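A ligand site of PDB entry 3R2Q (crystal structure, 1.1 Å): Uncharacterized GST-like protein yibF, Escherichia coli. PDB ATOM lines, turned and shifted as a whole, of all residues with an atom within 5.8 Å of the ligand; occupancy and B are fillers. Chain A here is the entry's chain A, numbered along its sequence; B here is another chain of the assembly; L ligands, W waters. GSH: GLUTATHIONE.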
ATOM      1  N   SER A   6      24.629  -5.383  26.973  1.00  0.00           N
ATOM      2  CA  SER A   6      23.477  -5.605  27.800  1.00  0.00           C
ATOM      3  C   SER A   6      23.888  -5.338  29.235  1.00  0.00           C
ATOM      4  O   SER A   6      25.089  -5.316  29.579  1.00  0.00           O
ATOM      5  CB  SER A   6      22.926  -6.991  27.593  1.00  0.00           C
ATOM      6  OG  SER A   6      23.782  -7.897  28.224  1.00  0.00           O
ATOM      7  N   SER A   9      25.319  -9.005  30.737  1.00  0.00           N
ATOM      8  CA  SER A   9      26.402  -9.815  30.167  1.00  0.00           C
ATOM      9  C   SER A   9      27.724  -9.631  30.874  1.00  0.00           C
ATOM     10  O   SER A   9      28.172  -8.475  31.012  1.00  0.00           O
ATOM     11  CB  SER A   9      26.596  -9.382  28.670  1.00  0.00           C
ATOM     12  OG  SER A   9      27.774  -9.988  28.159  1.00  0.00           O
ATOM     13  N   PRO A  10      28.403 -10.706  31.266  1.00  0.00           N
ATOM     14  CA  PRO A  10      29.707 -10.537  31.913  1.00  0.00           C
ATOM     15  C   PRO A  10      30.825 -10.208  30.937  1.00  0.00           C
ATOM     16  O   PRO A  10      31.853  -9.665  31.328  1.00  0.00           O
ATOM     17  CB  PRO A  10      29.887 -11.911  32.571  1.00  0.00           C
ATOM     18  CG  PRO A  10      29.175 -12.856  31.660  1.00  0.00           C
ATOM     19  CD  PRO A  10      27.947 -12.117  31.161  1.00  0.00           C
ATOM     20  N   PHE A  11      30.643 -10.577  29.655  1.00  0.00           N
ATOM     21  CA  PHE A  11      31.598 -10.200  28.638  1.00  0.00           C
ATOM     22  C   PHE A  11      31.632  -8.698  28.451  1.00  0.00           C
ATOM     23  O   PHE A  11      32.661  -8.076  28.280  1.00  0.00           O
ATOM     24  CB  PHE A  11      31.236 -10.866  27.293  1.00  0.00           C
ATOM     25  CG  PHE A  11      31.161 -12.381  27.347  1.00  0.00           C
ATOM     26  CD1 PHE A  11      32.335 -13.166  27.326  1.00  0.00           C
ATOM     27  CD2 PHE A  11      29.933 -13.004  27.370  1.00  0.00           C
ATOM     28  CE1 PHE A  11      32.207 -14.546  27.332  1.00  0.00           C
ATOM     29  CE2 PHE A  11      29.848 -14.369  27.407  1.00  0.00           C
ATOM     30  CZ  PHE A  11      30.990 -15.155  27.386  1.00  0.00           C
ATOM     31  N   LYS A  14      33.140  -6.961  31.779  1.00  0.00           N
ATOM     32  CA  LYS A  14      34.558  -6.930  31.803  1.00  0.00           C
ATOM     33  C   LYS A  14      35.108  -5.649  31.182  1.00  0.00           C
ATOM     34  O   LYS A  14      36.056  -5.035  31.672  1.00  0.00           O
ATOM     35  CB  LYS A  14      35.045  -8.198  31.028  1.00  0.00           C
ATOM     36  CG  LYS A  14      36.524  -8.294  30.781  1.00  0.00           C
ATOM     37  CD  LYS A  14      36.870  -9.570  30.050  1.00  0.00           C
ATOM     38  CE  LYS A  14      36.330  -9.717  28.663  1.00  0.00           C
ATOM     39  NZ  LYS A  14      36.841 -10.945  27.971  1.00  0.00           N
ATOM     40  N   PRO A  33      20.382  -9.090  22.909  1.00  0.00           N
ATOM     41  CA  PRO A  33      20.777  -9.865  21.736  1.00  0.00           C
ATOM     42  C   PRO A  33      19.961 -11.116  21.517  1.00  0.00           C
ATOM     43  O   PRO A  33      19.975 -11.665  20.444  1.00  0.00           O
ATOM     44  CB  PRO A  33      22.251 -10.202  21.995  1.00  0.00           C
ATOM     45  CG  PRO A  33      22.357 -10.167  23.468  1.00  0.00           C
ATOM     46  CD  PRO A  33      21.457  -9.053  23.945  1.00  0.00           C
ATOM     47  N   TYR A  34      19.223 -11.589  22.540  1.00  0.00           N
ATOM     48  CA  TYR A  34      18.338 -12.765  22.371  1.00  0.00           C
ATOM     49  C   TYR A  34      16.953 -12.378  22.021  1.00  0.00           C
ATOM     50  O   TYR A  34      16.130 -13.258  21.734  1.00  0.00           O
ATOM     51  CB  TYR A  34      18.361 -13.633  23.638  1.00  0.00           C
ATOM     52  CG  TYR A  34      19.708 -14.291  23.781  1.00  0.00           C
ATOM     53  CD1 TYR A  34      20.120 -15.370  22.951  1.00  0.00           C
ATOM     54  CD2 TYR A  34      20.608 -13.837  24.745  1.00  0.00           C
ATOM     55  CE1 TYR A  34      21.374 -15.941  23.127  1.00  0.00           C
ATOM     56  CE2 TYR A  34      21.865 -14.401  24.892  1.00  0.00           C
ATOM     57  CZ  TYR A  34      22.225 -15.451  24.061  1.00  0.00           C
ATOM     58  OH  TYR A  34      23.502 -15.943  24.305  1.00  0.00           O
ATOM     59  N   LEU A  46      27.702 -11.151  13.861  1.00  0.00           N
ATOM     60  CA  LEU A  46      27.469 -12.306  14.713  1.00  0.00           C
ATOM     61  C   LEU A  46      26.303 -12.097  15.655  1.00  0.00           C
ATOM     62  O   LEU A  46      25.880 -13.069  16.287  1.00  0.00           O
ATOM     63  CB  LEU A  46      28.718 -12.644  15.513  1.00  0.00           C
ATOM     64  CG  LEU A  46      29.953 -12.995  14.681  1.00  0.00           C
ATOM     65  CD1 LEU A  46      31.180 -13.015  15.583  1.00  0.00           C
ATOM     66  CD2 LEU A  46      29.772 -14.304  13.946  1.00  0.00           C
ATOM     67  N   GLY A  47      25.813 -10.870  15.823  1.00  0.00           N
ATOM     68  CA  GLY A  47      24.677 -10.627  16.676  1.00  0.00           C
ATOM     69  C   GLY A  47      24.992 -10.797  18.150  1.00  0.00           C
ATOM     70  O   GLY A  47      24.093 -11.111  18.928  1.00  0.00           O
ATOM     71  N   LYS A  48      26.240 -10.600  18.555  1.00  0.00           N
ATOM     72  CA  LYS A  48      26.640 -10.715  19.946  1.00  0.00           C
ATOM     73  C   LYS A  48      27.192  -9.394  20.464  1.00  0.00           C
ATOM     74  O   LYS A  48      27.778  -8.618  19.735  1.00  0.00           O
ATOM     75  CB  LYS A  48      27.698 -11.833  20.137  1.00  0.00           C
ATOM     76  CG  LYS A  48      27.158 -13.190  19.711  1.00  0.00           C
ATOM     77  CD  LYS A  48      28.027 -14.357  20.121  1.00  0.00           C
ATOM     78  CE  LYS A  48      27.497 -15.672  19.607  1.00  0.00           C
ATOM     79  NZ  LYS A  48      28.201 -16.811  20.178  1.00  0.00           N
ATOM     80  N   VAL A  49      26.982  -9.224  21.766  1.00  0.00           N
ATOM     81  CA  VAL A  49      27.603  -8.159  22.512  1.00  0.00           C
ATOM     82  C   VAL A  49      28.685  -8.730  23.412  1.00  0.00           C
ATOM     83  O   VAL A  49      28.575  -9.893  23.857  1.00  0.00           O
ATOM     84  CB  VAL A  49      26.577  -7.361  23.352  1.00  0.00           C
ATOM     85  CG1 VAL A  49      25.595  -6.644  22.412  1.00  0.00           C
ATOM     86  CG2 VAL A  49      25.894  -8.247  24.400  1.00  0.00           C
ATOM     87  N   PRO A  50      29.729  -7.977  23.740  1.00  0.00           N
ATOM     88  CA  PRO A  50      29.933  -6.559  23.444  1.00  0.00           C
ATOM     89  C   PRO A  50      30.437  -6.282  22.054  1.00  0.00           C
ATOM     90  O   PRO A  50      31.063  -7.101  21.374  1.00  0.00           O
ATOM     91  CB  PRO A  50      31.027  -6.161  24.453  1.00  0.00           C
ATOM     92  CG  PRO A  50      31.804  -7.457  24.640  1.00  0.00           C
ATOM     93  CD  PRO A  50      30.759  -8.518  24.639  1.00  0.00           C
ATOM     94  N   ASP A  62      35.493  -9.758  19.209  1.00  0.00           N
ATOM     95  CA  ASP A  62      34.726 -10.017  20.403  1.00  0.00           C
ATOM     96  C   ASP A  62      35.411  -9.444  21.637  1.00  0.00           C
ATOM     97  O   ASP A  62      36.348  -8.636  21.547  1.00  0.00           O
ATOM     98  CB  ASP A  62      34.383 -11.497  20.501  1.00  0.00           C
ATOM     99  CG  ASP A  62      35.561 -12.420  20.665  1.00  0.00           C
ATOM    100  OD1 ASP A  62      36.696 -12.037  20.241  1.00  0.00           O
ATOM    101  OD2 ASP A  62      35.344 -13.536  21.191  1.00  0.00           O
ATOM    102  N   SER A  63      34.940  -9.790  22.860  1.00  0.00           N
ATOM    103  CA  SER A  63      35.406  -9.123  24.039  1.00  0.00           C
ATOM    104  C   SER A  63      36.901  -9.171  24.271  1.00  0.00           C
ATOM    105  O   SER A  63      37.447  -8.135  24.705  1.00  0.00           O
ATOM    106  CB  SER A  63      34.658  -9.571  25.294  1.00  0.00           C
ATOM    107  OG  SER A  63      34.995 -10.851  25.767  1.00  0.00           O
ATOM    108  N   PRO A  64      37.643 -10.259  24.061  1.00  0.00           N
ATOM    109  CA  PRO A  64      39.086 -10.196  24.287  1.00  0.00           C
ATOM    110  C   PRO A  64      39.754  -9.219  23.347  1.00  0.00           C
ATOM    111  O   PRO A  64      40.730  -8.539  23.739  1.00  0.00           O
ATOM    112  CB  PRO A  64      39.566 -11.656  24.061  1.00  0.00           C
ATOM    113  CG  PRO A  64      38.378 -12.411  23.809  1.00  0.00           C
ATOM    114  CD  PRO A  64      37.219 -11.637  23.692  1.00  0.00           C
ATOM    115  N   ASP A  98      36.590 -16.347  30.415  1.00  0.00           N
ATOM    116  CA  ASP A  98      35.590 -16.207  29.399  1.00  0.00           C
ATOM    117  C   ASP A  98      34.890 -17.532  29.121  1.00  0.00           C
ATOM    118  O   ASP A  98      33.690 -17.552  28.827  1.00  0.00           O
ATOM    119  CB  ASP A  98      36.205 -15.694  28.114  1.00  0.00           C
ATOM    120  CG  ASP A  98      36.618 -14.218  28.158  1.00  0.00           C
ATOM    121  OD1 ASP A  98      36.283 -13.474  29.057  1.00  0.00           O
ATOM    122  OD2 ASP A  98      37.295 -13.794  27.160  1.00  0.00           O
ATOM    123  N   ASP A 102      31.060 -18.508  29.193  1.00  0.00           N
ATOM    124  CA  ASP A 102      30.417 -19.231  28.102  1.00  0.00           C
ATOM    125  C   ASP A 102      29.558 -20.379  28.660  1.00  0.00           C
ATOM    126  O   ASP A 102      28.422 -20.584  28.224  1.00  0.00           O
ATOM    127  CB  ASP A 102      31.432 -19.792  27.121  1.00  0.00           C
ATOM    128  CG  ASP A 102      32.269 -18.940  26.215  1.00  0.00           C
ATOM    129  OD1 ASP A 102      31.818 -17.823  25.914  1.00  0.00           O
ATOM    130  OD2 ASP A 102      33.363 -19.350  25.766  1.00  0.00           O
ATOM    131  N   LEU A 105      26.500 -19.137  30.447  1.00  0.00           N
ATOM    132  CA  LEU A 105      25.529 -18.659  29.474  1.00  0.00           C
ATOM    133  C   LEU A 105      24.820 -19.835  28.774  1.00  0.00           C
ATOM    134  O   LEU A 105      23.587 -19.813  28.616  1.00  0.00           O
ATOM    135  CB  LEU A 105      26.213 -17.757  28.453  1.00  0.00           C
ATOM    136  CG  LEU A 105      25.321 -17.216  27.363  1.00  0.00           C
ATOM    137  CD1 LEU A 105      24.187 -16.349  27.939  1.00  0.00           C
ATOM    138  CD2 LEU A 105      26.137 -16.437  26.336  1.00  0.00           C
ATOM    139  N   TYR A 164      28.681 -13.469  37.495  1.00  0.00           N
ATOM    140  CA  TYR A 164      27.650 -13.984  36.639  1.00  0.00           C
ATOM    141  C   TYR A 164      27.098 -15.312  37.153  1.00  0.00           C
ATOM    142  O   TYR A 164      25.901 -15.511  37.160  1.00  0.00           O
ATOM    143  CB  TYR A 164      28.181 -14.106  35.217  1.00  0.00           C
ATOM    144  CG  TYR A 164      27.124 -14.522  34.221  1.00  0.00           C
ATOM    145  CD1 TYR A 164      26.137 -13.622  33.838  1.00  0.00           C
ATOM    146  CD2 TYR A 164      27.106 -15.794  33.698  1.00  0.00           C
ATOM    147  CE1 TYR A 164      25.163 -14.018  32.909  1.00  0.00           C
ATOM    148  CE2 TYR A 164      26.141 -16.162  32.803  1.00  0.00           C
ATOM    149  CZ  TYR A 164      25.166 -15.270  32.392  1.00  0.00           C
ATOM    150  OH  TYR A 164      24.272 -15.789  31.527  1.00  0.00           O
ATOM    151  N   ASP B 102      31.699 -20.897  15.251  1.00  0.00           N
ATOM    152  CA  ASP B 102      30.862 -21.085  16.421  1.00  0.00           C
ATOM    153  C   ASP B 102      29.412 -21.358  16.008  1.00  0.00           C
ATOM    154  O   ASP B 102      28.749 -22.244  16.557  1.00  0.00           O
ATOM    155  CB  ASP B 102      30.914 -19.885  17.349  1.00  0.00           C
ATOM    156  CG  ASP B 102      32.130 -19.478  18.130  1.00  0.00           C
ATOM    157  OD1 ASP B 102      32.943 -20.375  18.409  1.00  0.00           O
ATOM    158  OD2 ASP B 102      32.298 -18.304  18.509  1.00  0.00           O
ATOM    159  N   ARG B 125      18.424 -18.782  13.711  1.00  0.00           N
ATOM    160  CA  ARG B 125      19.159 -17.571  14.105  1.00  0.00           C
ATOM    161  C   ARG B 125      20.648 -17.814  13.900  1.00  0.00           C
ATOM    162  O   ARG B 125      21.382 -16.844  13.610  1.00  0.00           O
ATOM    163  CB  ARG B 125      18.743 -17.163  15.487  1.00  0.00           C
ATOM    164  CG  ARG B 125      19.204 -18.027  16.630  1.00  0.00           C
ATOM    165  CD  ARG B 125      18.503 -17.596  17.917  1.00  0.00           C
ATOM    166  NE  ARG B 125      18.808 -16.207  18.337  1.00  0.00           N
ATOM    167  CZ  ARG B 125      19.929 -15.801  18.907  1.00  0.00           C
ATOM    168  NH1 ARG B 125      20.871 -16.709  19.164  1.00  0.00           N
ATOM    169  NH2 ARG B 125      20.169 -14.518  19.249  1.00  0.00           N
ATOM    170  N   GLN B 126      21.137 -19.054  14.007  1.00  0.00           N
ATOM    171  CA  GLN B 126      22.526 -19.325  13.670  1.00  0.00           C
ATOM    172  C   GLN B 126      22.797 -19.147  12.213  1.00  0.00           C
ATOM    173  O   GLN B 126      23.830 -18.583  11.793  1.00  0.00           O
ATOM    174  CB  GLN B 126      22.987 -20.698  14.163  1.00  0.00           C
ATOM    175  CG  GLN B 126      22.859 -20.873  15.671  1.00  0.00           C
ATOM    176  CD  GLN B 126      23.696 -19.937  16.494  1.00  0.00           C
ATOM    177  OE1 GLN B 126      24.811 -19.585  16.110  1.00  0.00           O
ATOM    178  NE2 GLN B 126      23.191 -19.500  17.658  1.00  0.00           N
ATOM    179  N   LYS B 129      23.186 -15.447  11.525  1.00  0.00           N
ATOM    180  CA  LYS B 129      24.484 -14.997  11.901  1.00  0.00           C
ATOM    181  C   LYS B 129      25.536 -15.303  10.820  1.00  0.00           C
ATOM    182  O   LYS B 129      26.378 -14.459  10.479  1.00  0.00           O
ATOM    183  CB  LYS B 129      24.976 -15.650  13.202  1.00  0.00           C
ATOM    184  CG  LYS B 129      24.171 -15.340  14.445  1.00  0.00           C
ATOM    185  CD  LYS B 129      24.737 -16.082  15.656  1.00  0.00           C
ATOM    186  CE  LYS B 129      23.910 -15.967  16.901  1.00  0.00           C
ATOM    187  NZ  LYS B 129      23.749 -14.583  17.383  1.00  0.00           N
HETATM  188  N1  GSH L   1      33.024 -14.560  22.313  1.00  0.00           N
HETATM  189  CA1 GSH L   1      32.137 -13.437  22.687  1.00  0.00           C
HETATM  190  C1  GSH L   1      32.885 -12.417  23.560  1.00  0.00           C
HETATM  191  O11 GSH L   1      32.495 -11.219  23.441  1.00  0.00           O
HETATM  192  O12 GSH L   1      33.818 -12.789  24.294  1.00  0.00           O
HETATM  193  CB1 GSH L   1      30.893 -14.006  23.415  1.00  0.00           C
HETATM  194  CG1 GSH L   1      29.865 -12.935  23.672  1.00  0.00           C
HETATM  195  CD1 GSH L   1      28.518 -13.488  24.086  1.00  0.00           C
HETATM  196  OE1 GSH L   1      28.301 -14.704  24.136  1.00  0.00           O
HETATM  197  N2  GSH L   1      27.595 -12.564  24.319  1.00  0.00           N
HETATM  198  CA2 GSH L   1      26.182 -12.970  24.569  1.00  0.00           C
HETATM  199  C2  GSH L   1      25.380 -12.619  23.326  1.00  0.00           C
HETATM  200  O2  GSH L   1      25.472 -11.535  22.751  1.00  0.00           O
HETATM  201  CB2 GSH L   1      25.568 -12.154  25.723  1.00  0.00           C
HETATM  202  SG2 GSH L   1      26.316 -12.589  27.295  1.00  0.00           S
HETATM  203  N3  GSH L   1      24.560 -13.637  22.945  1.00  0.00           N
HETATM  204  CA3 GSH L   1      23.667 -13.493  21.787  1.00  0.00           C
HETATM  205  C3  GSH L   1      23.709 -14.720  20.912  1.00  0.00           C
HETATM  206  O31 GSH L   1      22.903 -14.730  19.942  1.00  0.00           O
HETATM  207  O32 GSH L   1      24.521 -15.647  21.160  1.00  0.00           O
HETATM  208  O   HOH W   1      31.382  -9.898  21.188  1.00  0.00           O
HETATM  209  O   HOH W   2      26.802 -16.587  22.687  1.00  0.00           O
HETATM  210  O   HOH W   3      23.950 -18.271  23.158  1.00  0.00           O
HETATM  211  O   HOH W   4      31.992 -14.029  19.303  1.00  0.00           O
HETATM  212  O   HOH W   5      23.062 -10.408  27.299  1.00  0.00           O
HETATM  213  O   HOH W   6      35.575 -14.911  24.823  1.00  0.00           O
HETATM  214  O   HOH W   7      33.426 -16.260  24.493  1.00  0.00           O
HETATM  215  O   HOH W   8      32.277 -17.136  21.233  1.00  0.00           O
HETATM  216  O   HOH W   9      24.157 -18.061  20.096  1.00  0.00           O
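O31 of the ligand lies within salt-bridge range of NZ of Lys 129 of chain B (2.7 Å).
O11 of the ligand sits at hydrogen-bond distance from N of Ser 63 (2.9 Å).
An oxygen (O12) of the ligand is in hydrogen-bond range of the side-chain hydroxyl of Ser 63, 2.7 Å away.
N1 of the ligand lies within salt-bridge range of OD2 of Asp 62 (2.8 Å).
The guanidinium group (NH2) of Arg 125 of chain B is in salt-bridge range of an oxygen (O31) of the ligand, 2.8 Å away.
OH of Tyr 34 sits at hydrogen-bond distance from N3 of the ligand.
An oxygen (O2) of the ligand is in hydrogen-bond range of the backbone NH (N) of Val 49, at 2.9 Å.
The backbone carbonyl oxygen (O) of Val 49 lies within hydrogen-bond range of a nitrogen (N2) of the ligand (2.9 Å).
A sulfur (SG2) of the ligand lies close to the side-chain hydroxyl of Ser 9 (3.1 Å).
O32 of the ligand is in salt-bridge range of NZ of Lys 48 (3.98 Å).
NZ of Lys 129 of chain B is in hydrogen-bond range of O of Leu 46, at 2.8 Å.
The side-chain amino group (NZ) of Lys 14 lies within hydrogen-bond range of the side-chain hydroxyl (OG) of Ser 63 (2.9 Å).
The guanidinium group of Arg 125 of chain B lies within hydrogen-bond range of the backbone carbonyl oxygen of Pro 33, 3.1 Å away.
N of Phe 11 lies within hydrogen-bond range of OG of Ser 9 (3.3 Å).
The backbone NH of Ser 9 is in hydrogen-bond range of the side-chain hydroxyl of Ser 6.
Phe 11 touches the ligand.
Pro 33 touches the ligand.
Gly 47 touches the ligand (O to CA3, 3.7 Å).
Pro 50 touches the ligand (CD to O11, 3.4 Å).
CD of Pro 64 touches O12 of the ligand (3.6 Å).
CD2 of Leu 105 touches OE1 of the ligand (3.5 Å).
Hydrophobic or aromatic side chains that line the ligand: Phe 11, Pro 33, Tyr 34, Val 49, Pro 50, Pro 64 and Leu 105.
Of the 23 residues printed, 14 come within 4 Å of the ligand.
The nearest printed residue that does not touch the ligand is Pro 10 (4.2 Å).
Water W9 bridges an oxygen (O32) of the ligand (2.7 Å) and the side-chain amide nitrogen (NE2) of Gln 126 of chain B (3.0 Å).
Water W7 bridges OD1 of Asp 102 of chain A (2.7 Å) and N1 of the ligand (2.8 Å).
Water W6 lies within hydrogen-bond range of O12 of the ligand (2.8 Å) and OD2 of Asp 98 (3.1 Å).
Water W2 bridges an oxygen (OE1) of the ligand (2.8 Å) and the side-chain amino group (NZ) of Lys 48 (2.9 Å).
Water W1 bridges O of Pro 50 (2.8 Å) and O11 of the ligand (2.8 Å).
Water W3 lies within hydrogen-bond range of the side-chain hydroxyl (OH) of Tyr 34 (2.6 Å) and an oxygen (O32) of the ligand (3.3 Å).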
